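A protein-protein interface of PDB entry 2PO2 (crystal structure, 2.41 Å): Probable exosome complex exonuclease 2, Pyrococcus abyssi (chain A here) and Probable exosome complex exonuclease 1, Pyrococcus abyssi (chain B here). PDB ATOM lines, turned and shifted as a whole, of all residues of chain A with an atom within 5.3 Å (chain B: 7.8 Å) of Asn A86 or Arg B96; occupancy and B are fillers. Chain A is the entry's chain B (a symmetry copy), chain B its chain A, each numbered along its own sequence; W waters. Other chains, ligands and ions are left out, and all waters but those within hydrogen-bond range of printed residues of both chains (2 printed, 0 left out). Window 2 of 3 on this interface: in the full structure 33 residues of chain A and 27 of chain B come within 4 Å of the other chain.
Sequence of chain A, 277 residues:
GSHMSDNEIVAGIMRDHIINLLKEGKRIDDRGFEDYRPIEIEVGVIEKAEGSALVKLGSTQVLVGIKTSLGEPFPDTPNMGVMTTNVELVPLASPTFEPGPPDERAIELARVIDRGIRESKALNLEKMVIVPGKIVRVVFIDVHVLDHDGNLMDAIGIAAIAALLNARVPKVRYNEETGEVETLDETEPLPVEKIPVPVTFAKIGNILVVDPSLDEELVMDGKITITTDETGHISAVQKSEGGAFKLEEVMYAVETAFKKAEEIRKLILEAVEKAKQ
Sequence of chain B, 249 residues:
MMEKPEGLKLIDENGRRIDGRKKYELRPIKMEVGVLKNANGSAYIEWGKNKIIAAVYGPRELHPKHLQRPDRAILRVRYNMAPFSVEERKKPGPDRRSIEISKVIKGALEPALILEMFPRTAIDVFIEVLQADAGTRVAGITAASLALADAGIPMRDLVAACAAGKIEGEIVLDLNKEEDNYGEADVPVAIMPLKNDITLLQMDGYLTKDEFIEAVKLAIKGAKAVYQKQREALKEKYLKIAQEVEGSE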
ATOM      1  N   THR A  84     -24.276 -33.014  -3.313  1.00  0.00           N
ATOM      2  CA  THR A  84     -23.490 -32.599  -4.460  1.00  0.00           C
ATOM      3  C   THR A  84     -23.601 -33.700  -5.509  1.00  0.00           C
ATOM      4  O   THR A  84     -23.576 -34.895  -5.186  1.00  0.00           O
ATOM      5  CB  THR A  84     -22.070 -32.158  -4.023  1.00  0.00           C
ATOM      6  OG1 THR A  84     -21.285 -31.910  -5.163  1.00  0.00           O
ATOM      7  CG2 THR A  84     -21.383 -33.216  -3.247  1.00  0.00           C
ATOM      8  N   THR A  85     -23.863 -33.295  -6.742  1.00  0.00           N
ATOM      9  CA  THR A  85     -24.188 -34.218  -7.824  1.00  0.00           C
ATOM     10  C   THR A  85     -23.180 -34.059  -8.920  1.00  0.00           C
ATOM     11  O   THR A  85     -22.911 -32.958  -9.399  1.00  0.00           O
ATOM     12  CB  THR A  85     -25.571 -33.951  -8.397  1.00  0.00           C
ATOM     13  OG1 THR A  85     -26.559 -33.816  -7.332  1.00  0.00           O
ATOM     14  CG2 THR A  85     -25.940 -35.079  -9.360  1.00  0.00           C
ATOM     15  N   ASN A  86     -22.563 -35.167  -9.296  1.00  0.00           N
ATOM     16  CA  ASN A  86     -21.583 -35.161 -10.365  1.00  0.00           C
ATOM     17  C   ASN A  86     -21.959 -36.307 -11.291  1.00  0.00           C
ATOM     18  O   ASN A  86     -22.323 -37.407 -10.835  1.00  0.00           O
ATOM     19  CB  ASN A  86     -20.176 -35.323  -9.779  1.00  0.00           C
ATOM     20  CG  ASN A  86     -19.101 -35.032 -10.770  1.00  0.00           C
ATOM     21  OD1 ASN A  86     -18.389 -35.950 -11.253  1.00  0.00           O
ATOM     22  ND2 ASN A  86     -18.937 -33.745 -11.091  1.00  0.00           N
ATOM     23  N   VAL A  87     -21.945 -35.995 -12.589  1.00  0.00           N
ATOM     24  CA  VAL A  87     -22.062 -36.935 -13.707  1.00  0.00           C
ATOM     25  C   VAL A  87     -20.696 -37.094 -14.328  1.00  0.00           C
ATOM     26  O   VAL A  87     -20.101 -36.108 -14.768  1.00  0.00           O
ATOM     27  CB  VAL A  87     -22.978 -36.370 -14.752  1.00  0.00           C
ATOM     28  CG1 VAL A  87     -23.000 -37.268 -15.954  1.00  0.00           C
ATOM     29  CG2 VAL A  87     -24.428 -36.156 -14.158  1.00  0.00           C
ATOM     30  N   GLU A  88     -20.150 -38.328 -14.285  1.00  0.00           N
ATOM     31  CA  GLU A  88     -19.044 -38.678 -15.102  1.00  0.00           C
ATOM     32  C   GLU A  88     -19.561 -39.352 -16.350  1.00  0.00           C
ATOM     33  O   GLU A  88     -20.301 -40.339 -16.312  1.00  0.00           O
ATOM     34  CB  GLU A  88     -18.050 -39.563 -14.376  1.00  0.00           C
ATOM     35  CG  GLU A  88     -17.333 -38.878 -13.240  1.00  0.00           C
ATOM     36  CD  GLU A  88     -16.357 -37.805 -13.686  1.00  0.00           C
ATOM     37  OE1 GLU A  88     -16.565 -36.606 -13.400  1.00  0.00           O
ATOM     38  OE2 GLU A  88     -15.349 -38.156 -14.302  1.00  0.00           O
ATOM     39  N   PRO A 102     -15.685 -32.564 -16.217  1.00  0.00           N
ATOM     40  CA  PRO A 102     -16.982 -32.576 -16.931  1.00  0.00           C
ATOM     41  C   PRO A 102     -17.063 -31.617 -18.098  1.00  0.00           C
ATOM     42  O   PRO A 102     -16.601 -30.455 -17.997  1.00  0.00           O
ATOM     43  CB  PRO A 102     -17.970 -32.155 -15.849  1.00  0.00           C
ATOM     44  CG  PRO A 102     -17.493 -32.792 -14.618  1.00  0.00           C
ATOM     45  CD  PRO A 102     -15.905 -32.626 -14.749  1.00  0.00           C
ATOM     46  N   ILE A 107     -22.021 -31.500 -17.085  1.00  0.00           N
ATOM     47  CA  ILE A 107     -22.426 -30.385 -16.240  1.00  0.00           C
ATOM     48  C   ILE A 107     -23.899 -30.100 -16.375  1.00  0.00           C
ATOM     49  O   ILE A 107     -24.599 -30.030 -15.386  1.00  0.00           O
ATOM     50  CB  ILE A 107     -21.540 -29.122 -16.503  1.00  0.00           C
ATOM     51  CG1 ILE A 107     -20.143 -29.386 -15.914  1.00  0.00           C
ATOM     52  CG2 ILE A 107     -22.163 -27.920 -15.930  1.00  0.00           C
ATOM     53  CD1 ILE A 107     -19.021 -28.362 -16.287  1.00  0.00           C
ATOM     54  N   ALA A 110     -25.691 -33.083 -14.638  1.00  0.00           N
ATOM     55  CA  ALA A 110     -25.569 -33.006 -13.190  1.00  0.00           C
ATOM     56  C   ALA A 110     -26.490 -31.953 -12.608  1.00  0.00           C
ATOM     57  O   ALA A 110     -27.247 -32.228 -11.678  1.00  0.00           O
ATOM     58  CB  ALA A 110     -24.109 -32.757 -12.758  1.00  0.00           C
ATOM     59  N   ARG A 111     -26.434 -30.749 -13.142  1.00  0.00           N
ATOM     60  CA  ARG A 111     -27.185 -29.668 -12.567  1.00  0.00           C
ATOM     61  C   ARG A 111     -28.647 -29.897 -12.677  1.00  0.00           C
ATOM     62  O   ARG A 111     -29.354 -29.603 -11.742  1.00  0.00           O
ATOM     63  CB  ARG A 111     -26.818 -28.281 -13.143  1.00  0.00           C
ATOM     64  CG  ARG A 111     -25.400 -28.129 -13.277  1.00  0.00           C
ATOM     65  CD  ARG A 111     -24.857 -26.708 -13.159  1.00  0.00           C
ATOM     66  NE  ARG A 111     -25.766 -25.570 -13.142  1.00  0.00           N
ATOM     67  CZ  ARG A 111     -25.877 -24.735 -12.112  1.00  0.00           C
ATOM     68  NH1 ARG A 111     -25.166 -24.925 -11.023  1.00  0.00           N
ATOM     69  NH2 ARG A 111     -26.678 -23.682 -12.175  1.00  0.00           N
ATOM     70  N   ILE A 141     -23.752 -37.613  -4.824  1.00  0.00           N
ATOM     71  CA  ILE A 141     -24.396 -38.402  -5.857  1.00  0.00           C
ATOM     72  C   ILE A 141     -23.414 -38.438  -7.020  1.00  0.00           C
ATOM     73  O   ILE A 141     -23.162 -37.403  -7.680  1.00  0.00           O
ATOM     74  CB  ILE A 141     -25.710 -37.781  -6.287  1.00  0.00           C
ATOM     75  CG1 ILE A 141     -26.574 -37.525  -5.059  1.00  0.00           C
ATOM     76  CG2 ILE A 141     -26.385 -38.656  -7.348  1.00  0.00           C
ATOM     77  CD1 ILE A 141     -27.793 -36.894  -5.412  1.00  0.00           C
ATOM     78  N   ASP A 142     -22.793 -39.598  -7.224  1.00  0.00           N
ATOM     79  CA  ASP A 142     -21.825 -39.674  -8.251  1.00  0.00           C
ATOM     80  C   ASP A 142     -22.407 -40.557  -9.263  1.00  0.00           C
ATOM     81  O   ASP A 142     -22.738 -41.691  -8.957  1.00  0.00           O
ATOM     82  CB  ASP A 142     -20.492 -40.199  -7.745  1.00  0.00           C
ATOM     83  CG  ASP A 142     -19.876 -39.264  -6.808  1.00  0.00           C
ATOM     84  OD1 ASP A 142     -19.659 -39.710  -5.664  1.00  0.00           O
ATOM     85  OD2 ASP A 142     -19.656 -38.052  -7.174  1.00  0.00           O
ATOM     86  N   VAL A 143     -22.496 -40.049 -10.476  1.00  0.00           N
ATOM     87  CA  VAL A 143     -23.239 -40.717 -11.496  1.00  0.00           C
ATOM     88  C   VAL A 143     -22.212 -41.158 -12.482  1.00  0.00           C
ATOM     89  O   VAL A 143     -21.534 -40.318 -13.079  1.00  0.00           O
ATOM     90  CB  VAL A 143     -24.208 -39.757 -12.238  1.00  0.00           C
ATOM     91  CG1 VAL A 143     -24.705 -40.412 -13.474  1.00  0.00           C
ATOM     92  CG2 VAL A 143     -25.309 -39.252 -11.317  1.00  0.00           C
ATOM     93  N   GLY B  93     -13.083 -17.317 -14.049  1.00  0.00           N
ATOM     94  CA  GLY B  93     -13.015 -18.561 -14.793  1.00  0.00           C
ATOM     95  C   GLY B  93     -14.380 -19.189 -14.997  1.00  0.00           C
ATOM     96  O   GLY B  93     -15.402 -18.608 -14.632  1.00  0.00           O
ATOM     97  N   PRO B  94     -14.396 -20.381 -15.584  1.00  0.00           N
ATOM     98  CA  PRO B  94     -15.645 -21.120 -15.795  1.00  0.00           C
ATOM     99  C   PRO B  94     -16.091 -21.851 -14.533  1.00  0.00           C
ATOM    100  O   PRO B  94     -15.254 -22.363 -13.790  1.00  0.00           O
ATOM    101  CB  PRO B  94     -15.269 -22.129 -16.882  1.00  0.00           C
ATOM    102  CG  PRO B  94     -14.172 -21.467 -17.638  1.00  0.00           C
ATOM    103  CD  PRO B  94     -13.395 -20.674 -16.624  1.00  0.00           C
ATOM    104  N   ASP B  95     -17.398 -21.894 -14.300  1.00  0.00           N
ATOM    105  CA  ASP B  95     -17.959 -22.787 -13.344  1.00  0.00           C
ATOM    106  C   ASP B  95     -19.149 -23.490 -13.916  1.00  0.00           C
ATOM    107  O   ASP B  95     -19.596 -23.127 -14.936  1.00  0.00           O
ATOM    108  CB  ASP B  95     -18.238 -22.085 -12.013  1.00  0.00           C
ATOM    109  CG  ASP B  95     -19.255 -20.977 -12.100  1.00  0.00           C
ATOM    110  OD1 ASP B  95     -19.500 -20.367 -11.082  1.00  0.00           O
ATOM    111  OD2 ASP B  95     -19.803 -20.685 -13.126  1.00  0.00           O
ATOM    112  N   ARG B  96     -19.597 -24.539 -13.265  1.00  0.00           N
ATOM    113  CA  ARG B  96     -20.698 -25.361 -13.723  1.00  0.00           C
ATOM    114  C   ARG B  96     -21.830 -24.497 -14.119  1.00  0.00           C
ATOM    115  O   ARG B  96     -22.304 -24.635 -15.194  1.00  0.00           O
ATOM    116  CB  ARG B  96     -21.108 -26.385 -12.662  1.00  0.00           C
ATOM    117  CG  ARG B  96     -19.957 -26.728 -11.809  1.00  0.00           C
ATOM    118  CD  ARG B  96     -19.677 -28.140 -11.828  1.00  0.00           C
ATOM    119  NE  ARG B  96     -20.902 -28.851 -11.539  1.00  0.00           N
ATOM    120  CZ  ARG B  96     -21.014 -30.163 -11.703  1.00  0.00           C
ATOM    121  NH1 ARG B  96     -19.963 -30.860 -12.164  1.00  0.00           N
ATOM    122  NH2 ARG B  96     -22.162 -30.757 -11.415  1.00  0.00           N
ATOM    123  N   ARG B  97     -22.217 -23.551 -13.279  1.00  0.00           N
ATOM    124  CA  ARG B  97     -23.276 -22.620 -13.639  1.00  0.00           C
ATOM    125  C   ARG B  97     -23.067 -21.970 -14.968  1.00  0.00           C
ATOM    126  O   ARG B  97     -23.916 -22.101 -15.796  1.00  0.00           O
ATOM    127  CB  ARG B  97     -23.501 -21.517 -12.589  1.00  0.00           C
ATOM    128  CG  ARG B  97     -24.817 -20.735 -12.775  1.00  0.00           C
ATOM    129  CD  ARG B  97     -24.822 -19.454 -11.957  1.00  0.00           C
ATOM    130  NE  ARG B  97     -24.629 -18.199 -12.702  1.00  0.00           N
ATOM    131  CZ  ARG B  97     -25.699 -17.468 -12.944  1.00  0.00           C
ATOM    132  NH1 ARG B  97     -25.702 -16.299 -13.590  1.00  0.00           N
ATOM    133  NH2 ARG B  97     -26.822 -17.975 -12.477  1.00  0.00           N
ATOM    134  N   SER B  98     -21.976 -21.242 -15.172  1.00  0.00           N
ATOM    135  CA  SER B  98     -21.730 -20.516 -16.415  1.00  0.00           C
ATOM    136  C   SER B  98     -21.649 -21.440 -17.626  1.00  0.00           C
ATOM    137  O   SER B  98     -21.897 -21.048 -18.757  1.00  0.00           O
ATOM    138  CB  SER B  98     -20.429 -19.729 -16.295  1.00  0.00           C
ATOM    139  OG  SER B  98     -19.345 -20.597 -15.994  1.00  0.00           O
ATOM    140  N   ILE B  99     -21.296 -22.700 -17.382  1.00  0.00           N
ATOM    141  CA  ILE B  99     -21.098 -23.645 -18.457  1.00  0.00           C
ATOM    142  C   ILE B  99     -22.417 -24.141 -18.884  1.00  0.00           C
ATOM    143  O   ILE B  99     -22.653 -24.318 -20.091  1.00  0.00           O
ATOM    144  CB  ILE B  99     -20.173 -24.807 -18.030  1.00  0.00           C
ATOM    145  CG1 ILE B  99     -18.741 -24.359 -18.163  1.00  0.00           C
ATOM    146  CG2 ILE B  99     -20.515 -26.085 -18.753  1.00  0.00           C
ATOM    147  CD1 ILE B  99     -17.899 -24.950 -17.158  1.00  0.00           C
ATOM    148  N   GLU B 100     -23.293 -24.394 -17.920  1.00  0.00           N
ATOM    149  CA  GLU B 100     -24.651 -24.757 -18.290  1.00  0.00           C
ATOM    150  C   GLU B 100     -25.338 -23.573 -18.918  1.00  0.00           C
ATOM    151  O   GLU B 100     -26.056 -23.736 -19.872  1.00  0.00           O
ATOM    152  CB  GLU B 100     -25.462 -25.285 -17.108  1.00  0.00           C
ATOM    153  CG  GLU B 100     -26.964 -25.473 -17.436  1.00  0.00           C
ATOM    154  CD  GLU B 100     -27.860 -25.493 -16.215  1.00  0.00           C
ATOM    155  OE1 GLU B 100     -27.411 -25.267 -15.077  1.00  0.00           O
ATOM    156  OE2 GLU B 100     -29.061 -25.731 -16.393  1.00  0.00           O
ATOM    157  N   ILE B 101     -25.117 -22.363 -18.426  1.00  0.00           N
ATOM    158  CA  ILE B 101     -25.820 -21.183 -18.987  1.00  0.00           C
ATOM    159  C   ILE B 101     -25.325 -20.993 -20.436  1.00  0.00           C
ATOM    160  O   ILE B 101     -26.079 -20.729 -21.354  1.00  0.00           O
ATOM    161  CB  ILE B 101     -25.594 -19.950 -18.111  1.00  0.00           C
ATOM    162  CG1 ILE B 101     -26.283 -20.078 -16.762  1.00  0.00           C
ATOM    163  CG2 ILE B 101     -26.014 -18.709 -18.764  1.00  0.00           C
ATOM    164  CD1 ILE B 101     -26.288 -18.729 -16.026  1.00  0.00           C
ATOM    165  N   SER B 102     -24.046 -21.196 -20.648  1.00  0.00           N
ATOM    166  CA  SER B 102     -23.505 -21.143 -22.009  1.00  0.00           C
ATOM    167  C   SER B 102     -24.178 -22.168 -22.940  1.00  0.00           C
ATOM    168  O   SER B 102     -24.446 -21.858 -24.098  1.00  0.00           O
ATOM    169  CB  SER B 102     -21.994 -21.404 -21.961  1.00  0.00           C
ATOM    170  OG  SER B 102     -21.405 -20.335 -21.281  1.00  0.00           O
ATOM    171  N   LYS B 103     -24.428 -23.382 -22.436  1.00  0.00           N
ATOM    172  CA  LYS B 103     -24.970 -24.452 -23.253  1.00  0.00           C
ATOM    173  C   LYS B 103     -26.398 -24.111 -23.641  1.00  0.00           C
ATOM    174  O   LYS B 103     -26.850 -24.341 -24.765  1.00  0.00           O
ATOM    175  CB  LYS B 103     -24.897 -25.793 -22.516  1.00  0.00           C
ATOM    176  CG  LYS B 103     -25.168 -26.950 -23.411  1.00  0.00           C
ATOM    177  CD  LYS B 103     -25.086 -28.255 -22.693  1.00  0.00           C
ATOM    178  CE  LYS B 103     -25.370 -29.462 -23.584  1.00  0.00           C
ATOM    179  NZ  LYS B 103     -26.886 -29.458 -23.892  1.00  0.00           N
HETATM  180  O   HOH W   1     -20.789 -33.430 -13.743  1.00  0.00           O
HETATM  181  O   HOH W   2     -24.101 -30.208 -10.046  1.00  0.00           O
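Asn A86 touches just one residue of chain B: Arg B96 (3.2 Å). Of the printed residues of chain A, Arg B96 touches Thr A85, Asn A86, Pro A102, Ile A107, Ala A110 and Arg A111. Of the printed residues of chain B, Ala A110 touches Arg B96 (3.1 Å). Printed residues of chain B within 4 Å of Pro A102: Arg B96 (3.98 Å). Printed residues of chain A within 4 Å of Glu B100: Arg A111 (2.6 Å). Of the printed residues of chain A, Ile B99 touches Ile A107. Lys B103 touches none of the printed residues of chain A. The nearest printed residue of chain B that does not touch Asn A86 is Asp B95 (10.6 Å). The nearest printed residue of chain B that does not touch Ile A107 is Glu B100 (4.2 Å).
Arg B96 touches Pro A102 (NH1 to CG, 3.98 Å). CG2 of Ile A107 touches O of Arg B96, at 3.4 Å. CD1 of Ile A107 touches CG2 of Ile B99, 3.7 Å away. Ala A110 touches Arg B96 (CB to NH2, 3.1 Å). CB of Arg B96 touches CD of Arg A111, at 3.8 Å. Arg B97 touches Arg A111.
The side-chain carboxylate (OE1) of Glu A88 sits close to the side-chain amide oxygen (OD1) of Asn A86, 2.9 Å away. O of Ile A141 is in hydrogen-bond range of N of Asn A86 (2.8 Å). N of Val A143 lies within hydrogen-bond range of O of Asn A86 (2.7 Å).
Hydrophobic or aromatic side chains of chain B within 4 Å of the printed part of chain A: Ile B99. Along chain B the printed residues that touch a printed residue of chain A span positions 96 to 100. Of the 12 printed residues of chain A, 6 touch a printed residue of chain B. Among the printed residues, Asp or Glu carboxylates within 4 Å of a Lys or Arg side-chain nitrogen of the other chain: Arg A111 with Glu B100.
The guanidinium group (NH2) of Arg B96 is in hydrogen-bond range of the backbone carbonyl oxygen (O) of Thr A85, 3.1 Å away. The guanidinium group of Arg B96 lies close to the side-chain amide nitrogen of Asn A86 (3.2 Å). The side-chain carboxylate (OE1) of Glu B100 is in salt-bridge range of the guanidinium group (NE) of Arg A111 (2.6 Å).
Water W2 lies within hydrogen-bond range of NH2 of Arg B96 (2.4 Å) and O of Thr A85 (3.1 Å). Water W1 lies within hydrogen-bond range of the backbone carbonyl oxygen of Val A87 (2.9 Å), the guanidinium group of Arg B96 (3.1 Å) and the side-chain amide nitrogen of Asn A86 (3.2 Å).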
